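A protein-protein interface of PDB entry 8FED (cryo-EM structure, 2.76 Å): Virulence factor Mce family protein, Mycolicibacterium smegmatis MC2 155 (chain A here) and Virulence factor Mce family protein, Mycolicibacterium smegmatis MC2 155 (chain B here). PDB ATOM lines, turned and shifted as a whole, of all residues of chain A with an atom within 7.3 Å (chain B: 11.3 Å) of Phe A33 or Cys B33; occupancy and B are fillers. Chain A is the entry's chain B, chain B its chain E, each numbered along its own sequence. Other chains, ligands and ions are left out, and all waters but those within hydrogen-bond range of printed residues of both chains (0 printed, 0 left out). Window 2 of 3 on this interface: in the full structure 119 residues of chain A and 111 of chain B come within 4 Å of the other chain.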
ATOM      1  N   ALA A  22       5.407 -32.191 -18.268  1.00  0.00           N
ATOM      2  CA  ALA A  22       6.226 -31.157 -17.645  1.00  0.00           C
ATOM      3  C   ALA A  22       6.316 -31.360 -16.139  1.00  0.00           C
ATOM      4  O   ALA A  22       7.358 -31.089 -15.535  1.00  0.00           O
ATOM      5  CB  ALA A  22       5.663 -29.775 -17.970  1.00  0.00           C
ATOM      6  N   VAL A  26       9.721 -31.754 -14.037  1.00  0.00           N
ATOM      7  CA  VAL A  26      10.022 -30.944 -12.858  1.00  0.00           C
ATOM      8  C   VAL A  26      10.315 -31.834 -11.655  1.00  0.00           C
ATOM      9  O   VAL A  26      11.261 -31.587 -10.898  1.00  0.00           O
ATOM     10  CB  VAL A  26       8.866 -29.966 -12.574  1.00  0.00           C
ATOM     11  CG1 VAL A  26       9.020 -29.331 -11.205  1.00  0.00           C
ATOM     12  CG2 VAL A  26       8.807 -28.895 -13.648  1.00  0.00           C
ATOM     13  N   ILE A  31      13.574 -29.241 -10.411  1.00  0.00           N
ATOM     14  CA  ILE A  31      13.486 -27.884 -10.937  1.00  0.00           C
ATOM     15  C   ILE A  31      12.922 -26.974  -9.855  1.00  0.00           C
ATOM     16  O   ILE A  31      11.879 -27.271  -9.260  1.00  0.00           O
ATOM     17  CB  ILE A  31      12.617 -27.842 -12.206  1.00  0.00           C
ATOM     18  CG1 ILE A  31      13.183 -28.781 -13.271  1.00  0.00           C
ATOM     19  CG2 ILE A  31      12.539 -26.428 -12.749  1.00  0.00           C
ATOM     20  CD1 ILE A  31      14.569 -28.408 -13.739  1.00  0.00           C
ATOM     21  N   ARG A  32      13.612 -25.865  -9.599  1.00  0.00           N
ATOM     22  CA  ARG A  32      13.189 -24.881  -8.615  1.00  0.00           C
ATOM     23  C   ARG A  32      12.905 -23.552  -9.299  1.00  0.00           C
ATOM     24  O   ARG A  32      13.514 -23.215 -10.319  1.00  0.00           O
ATOM     25  CB  ARG A  32      14.252 -24.685  -7.524  1.00  0.00           C
ATOM     26  CG  ARG A  32      14.004 -25.474  -6.247  1.00  0.00           C
ATOM     27  CD  ARG A  32      14.029 -26.968  -6.502  1.00  0.00           C
ATOM     28  NE  ARG A  32      13.807 -27.740  -5.286  1.00  0.00           N
ATOM     29  CZ  ARG A  32      13.847 -29.063  -5.225  1.00  0.00           C
ATOM     30  NH1 ARG A  32      14.099 -29.796  -6.296  1.00  0.00           N
ATOM     31  NH2 ARG A  32      13.636 -29.666  -4.060  1.00  0.00           N
ATOM     32  N   PHE A  33      11.976 -22.792  -8.720  1.00  0.00           N
ATOM     33  CA  PHE A  33      11.543 -21.529  -9.303  1.00  0.00           C
ATOM     34  C   PHE A  33      11.696 -20.384  -8.311  1.00  0.00           C
ATOM     35  O   PHE A  33      10.769 -19.591  -8.126  1.00  0.00           O
ATOM     36  CB  PHE A  33      10.089 -21.623  -9.767  1.00  0.00           C
ATOM     37  CG  PHE A  33       9.790 -22.846 -10.583  1.00  0.00           C
ATOM     38  CD1 PHE A  33      10.137 -22.903 -11.921  1.00  0.00           C
ATOM     39  CD2 PHE A  33       9.158 -23.936 -10.012  1.00  0.00           C
ATOM     40  CE1 PHE A  33       9.861 -24.026 -12.673  1.00  0.00           C
ATOM     41  CE2 PHE A  33       8.881 -25.062 -10.759  1.00  0.00           C
ATOM     42  CZ  PHE A  33       9.233 -25.107 -12.091  1.00  0.00           C
ATOM     43  N   ASN A  34      12.856 -20.289  -7.668  1.00  0.00           N
ATOM     44  CA  ASN A  34      13.120 -19.253  -6.682  1.00  0.00           C
ATOM     45  C   ASN A  34      14.306 -18.401  -7.116  1.00  0.00           C
ATOM     46  O   ASN A  34      15.214 -18.876  -7.806  1.00  0.00           O
ATOM     47  CB  ASN A  34      13.391 -19.857  -5.299  1.00  0.00           C
ATOM     48  CG  ASN A  34      14.611 -20.757  -5.284  1.00  0.00           C
ATOM     49  OD1 ASN A  34      14.987 -21.329  -6.306  1.00  0.00           O
ATOM     50  ND2 ASN A  34      15.236 -20.887  -4.120  1.00  0.00           N
ATOM     51  N   ARG A  35      14.279 -17.133  -6.714  1.00  0.00           N
ATOM     52  CA  ARG A  35      15.392 -16.233  -6.979  1.00  0.00           C
ATOM     53  C   ARG A  35      16.554 -16.561  -6.051  1.00  0.00           C
ATOM     54  O   ARG A  35      16.376 -16.677  -4.835  1.00  0.00           O
ATOM     55  CB  ARG A  35      14.944 -14.782  -6.802  1.00  0.00           C
ATOM     56  CG  ARG A  35      13.897 -14.352  -7.820  1.00  0.00           C
ATOM     57  CD  ARG A  35      13.156 -13.085  -7.409  1.00  0.00           C
ATOM     58  NE  ARG A  35      14.018 -11.912  -7.341  1.00  0.00           N
ATOM     59  CZ  ARG A  35      14.339 -11.282  -6.219  1.00  0.00           C
ATOM     60  NH1 ARG A  35      13.881 -11.684  -5.045  1.00  0.00           N
ATOM     61  NH2 ARG A  35      15.129 -10.214  -6.278  1.00  0.00           N
ATOM     62  N   THR A  36      17.746 -16.714  -6.624  1.00  0.00           N
ATOM     63  CA  THR A  36      18.901 -17.204  -5.887  1.00  0.00           C
ATOM     64  C   THR A  36      20.080 -16.255  -6.051  1.00  0.00           C
ATOM     65  O   THR A  36      20.180 -15.507  -7.027  1.00  0.00           O
ATOM     66  CB  THR A  36      19.309 -18.611  -6.347  1.00  0.00           C
ATOM     67  OG1 THR A  36      19.558 -18.601  -7.757  1.00  0.00           O
ATOM     68  CG2 THR A  36      18.215 -19.620  -6.036  1.00  0.00           C
ATOM     69  N   CYS B  33       4.481 -22.683  -6.819  1.00  0.00           N
ATOM     70  CA  CYS B  33       5.455 -22.313  -7.839  1.00  0.00           C
ATOM     71  C   CYS B  33       6.696 -21.689  -7.209  1.00  0.00           C
ATOM     72  O   CYS B  33       7.797 -22.227  -7.323  1.00  0.00           O
ATOM     73  CB  CYS B  33       4.835 -21.346  -8.848  1.00  0.00           C
ATOM     74  SG  CYS B  33       5.945 -20.840 -10.182  1.00  0.00           S
ATOM     75  N   GLY B  34       6.509 -20.545  -6.549  1.00  0.00           N
ATOM     76  CA  GLY B  34       7.630 -19.884  -5.902  1.00  0.00           C
ATOM     77  C   GLY B  34       8.179 -20.668  -4.725  1.00  0.00           C
ATOM     78  O   GLY B  34       9.393 -20.716  -4.512  1.00  0.00           O
ATOM     79  N   GLN B  35       7.296 -21.294  -3.948  1.00  0.00           N
ATOM     80  CA  GLN B  35       7.680 -22.026  -2.750  1.00  0.00           C
ATOM     81  C   GLN B  35       7.844 -23.519  -2.999  1.00  0.00           C
ATOM     82  O   GLN B  35       7.923 -24.290  -2.039  1.00  0.00           O
ATOM     83  CB  GLN B  35       6.651 -21.797  -1.642  1.00  0.00           C
ATOM     84  CG  GLN B  35       5.246 -22.248  -2.006  1.00  0.00           C
ATOM     85  CD  GLN B  35       4.254 -22.037  -0.879  1.00  0.00           C
ATOM     86  OE1 GLN B  35       4.627 -21.653   0.229  1.00  0.00           O
ATOM     87  NE2 GLN B  35       2.980 -22.289  -1.159  1.00  0.00           N
ATOM     88  N   TRP B  36       7.883 -23.941  -4.261  1.00  0.00           N
ATOM     89  CA  TRP B  36       8.034 -25.352  -4.602  1.00  0.00           C
ATOM     90  C   TRP B  36       9.401 -25.846  -4.144  1.00  0.00           C
ATOM     91  O   TRP B  36      10.429 -25.472  -4.717  1.00  0.00           O
ATOM     92  CB  TRP B  36       7.856 -25.549  -6.104  1.00  0.00           C
ATOM     93  CG  TRP B  36       8.235 -26.915  -6.586  1.00  0.00           C
ATOM     94  CD1 TRP B  36       9.414 -27.283  -7.162  1.00  0.00           C
ATOM     95  CD2 TRP B  36       7.430 -28.097  -6.529  1.00  0.00           C
ATOM     96  NE1 TRP B  36       9.393 -28.621  -7.471  1.00  0.00           N
ATOM     97  CE2 TRP B  36       8.185 -29.143  -7.091  1.00  0.00           C
ATOM     98  CE3 TRP B  36       6.143 -28.372  -6.058  1.00  0.00           C
ATOM     99  CZ2 TRP B  36       7.696 -30.442  -7.196  1.00  0.00           C
ATOM    100  CZ3 TRP B  36       5.661 -29.661  -6.162  1.00  0.00           C
ATOM    101  CH2 TRP B  36       6.435 -30.679  -6.728  1.00  0.00           C
ATOM    102  N   ARG B  37       9.413 -26.689  -3.115  1.00  0.00           N
ATOM    103  CA  ARG B  37      10.642 -27.263  -2.588  1.00  0.00           C
ATOM    104  C   ARG B  37      10.853 -28.709  -3.013  1.00  0.00           C
ATOM    105  O   ARG B  37      11.840 -29.323  -2.597  1.00  0.00           O
ATOM    106  CB  ARG B  37      10.661 -27.164  -1.060  1.00  0.00           C
ATOM    107  CG  ARG B  37      11.766 -26.269  -0.526  1.00  0.00           C
ATOM    108  CD  ARG B  37      11.686 -24.884  -1.146  1.00  0.00           C
ATOM    109  NE  ARG B  37      12.845 -24.063  -0.818  1.00  0.00           N
ATOM    110  CZ  ARG B  37      12.998 -22.801  -1.197  1.00  0.00           C
ATOM    111  NH1 ARG B  37      12.079 -22.181  -1.918  1.00  0.00           N
ATOM    112  NH2 ARG B  37      14.100 -22.146  -0.843  1.00  0.00           N
ATOM    113  N   GLY B  38       9.960 -29.265  -3.825  1.00  0.00           N
ATOM    114  CA  GLY B  38      10.138 -30.613  -4.323  1.00  0.00           C
ATOM    115  C   GLY B  38       8.983 -31.534  -3.997  1.00  0.00           C
ATOM    116  O   GLY B  38       8.164 -31.232  -3.125  1.00  0.00           O
ATOM    117  N   ILE B  39       8.906 -32.663  -4.705  1.00  0.00           N
ATOM    118  CA  ILE B  39       7.850 -33.638  -4.452  1.00  0.00           C
ATOM    119  C   ILE B  39       7.997 -34.248  -3.061  1.00  0.00           C
ATOM    120  O   ILE B  39       7.008 -34.670  -2.451  1.00  0.00           O
ATOM    121  CB  ILE B  39       7.852 -34.711  -5.560  1.00  0.00           C
ATOM    122  CG1 ILE B  39       6.653 -35.649  -5.419  1.00  0.00           C
ATOM    123  CG2 ILE B  39       9.159 -35.493  -5.559  1.00  0.00           C
ATOM    124  CD1 ILE B  39       5.320 -34.949  -5.514  1.00  0.00           C
ATOM    125  N   ASN B  41       8.821 -32.649  -0.353  1.00  0.00           N
ATOM    126  CA  ASN B  41       8.539 -31.665   0.685  1.00  0.00           C
ATOM    127  C   ASN B  41       7.121 -31.108   0.610  1.00  0.00           C
ATOM    128  O   ASN B  41       6.835 -30.077   1.226  1.00  0.00           O
ATOM    129  CB  ASN B  41       9.556 -30.525   0.614  1.00  0.00           C
ATOM    130  CG  ASN B  41      10.960 -30.980   0.951  1.00  0.00           C
ATOM    131  OD1 ASN B  41      11.170 -31.723   1.907  1.00  0.00           O
ATOM    132  ND2 ASN B  41      11.930 -30.538   0.160  1.00  0.00           N
ATOM    133  N   VAL B  42       6.228 -31.756  -0.130  1.00  0.00           N
ATOM    134  CA  VAL B  42       4.840 -31.303  -0.208  1.00  0.00           C
ATOM    135  C   VAL B  42       4.011 -32.124   0.774  1.00  0.00           C
ATOM    136  O   VAL B  42       4.229 -33.338   0.902  1.00  0.00           O
ATOM    137  CB  VAL B  42       4.305 -31.394  -1.649  1.00  0.00           C
ATOM    138  CG1 VAL B  42       4.439 -32.801  -2.201  1.00  0.00           C
ATOM    139  CG2 VAL B  42       2.860 -30.926  -1.733  1.00  0.00           C
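The guanidinium group (NH2) of Arg A32 sits close to the backbone carbonyl oxygen (O) of Arg B37 (2.3 Å).
The indole nitrogen (NE1) of Trp B36 lies close to the backbone carbonyl oxygen (O) of Ile A31, 3.3 Å away.
O of Val A26 is in hydrogen-bond range of N of Ile A31 (3.3 Å).
O of Arg B37 sits at hydrogen-bond distance from ND2 of Asn B41 (3.0 Å).
Trp B36 touches Val A26 (NE1 to CG1, 3.8 Å).
Arg A32 touches Trp B36.
Gly B38 touches Arg A32 (CA to NH2, 3.6 Å).
Phe A33 touches Cys B33 (CB to O, 3.4 Å).
O of Phe A33 touches CA of Gly B34 (3.9 Å).
Asn A34 touches Arg B37.
Val A26 touches one residue of chain B.
Ile A31 touches just one residue of chain B: Trp B36 (3.2 Å).
Of chain B, only Cys B33 (3.4 Å) and Gly B34 (3.9 Å) come within 4 Å of Phe A33.
Of chain B, only Arg B37 (3.7 Å) comes within 4 Å of Asn A34.
Printed residues of chain A within 4 Å of Cys B33: Phe A33.
Of the printed residues of chain A, Gly B34 touches Phe A33 (3.9 Å).
Printed residues of chain A within 4 Å of Trp B36: Val A26 (3.8 Å), Ile A31 (3.2 Å) and Arg A32 (3.9 Å).
Of the printed residues of chain A, Arg B37 touches Arg A32 (2.3 Å) and Asn A34 (3.7 Å).
Printed residues of chain A within 4 Å of Gly B38: Arg A32 (3.6 Å).
The nearest residue of chain A that does not touch Cys B33 is Asn A34 (5.4 Å).
The nearest printed residue of chain B that does not touch Arg A32 is Asn B41 (4.6 Å).
Hydrophobic or aromatic side chains of chain B that line the printed part of chain A: Trp B36.
Printed residues of chain A that touch a printed residue of chain B: Val A26, Ile A31, Arg A32, Phe A33 and Asn A34.
Hydrophobic or aromatic side chains of chain A within 4 Å of the printed part of chain B: Val A26 and Phe A33.
Among the printed residues, 8 pairs touch across the chains.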
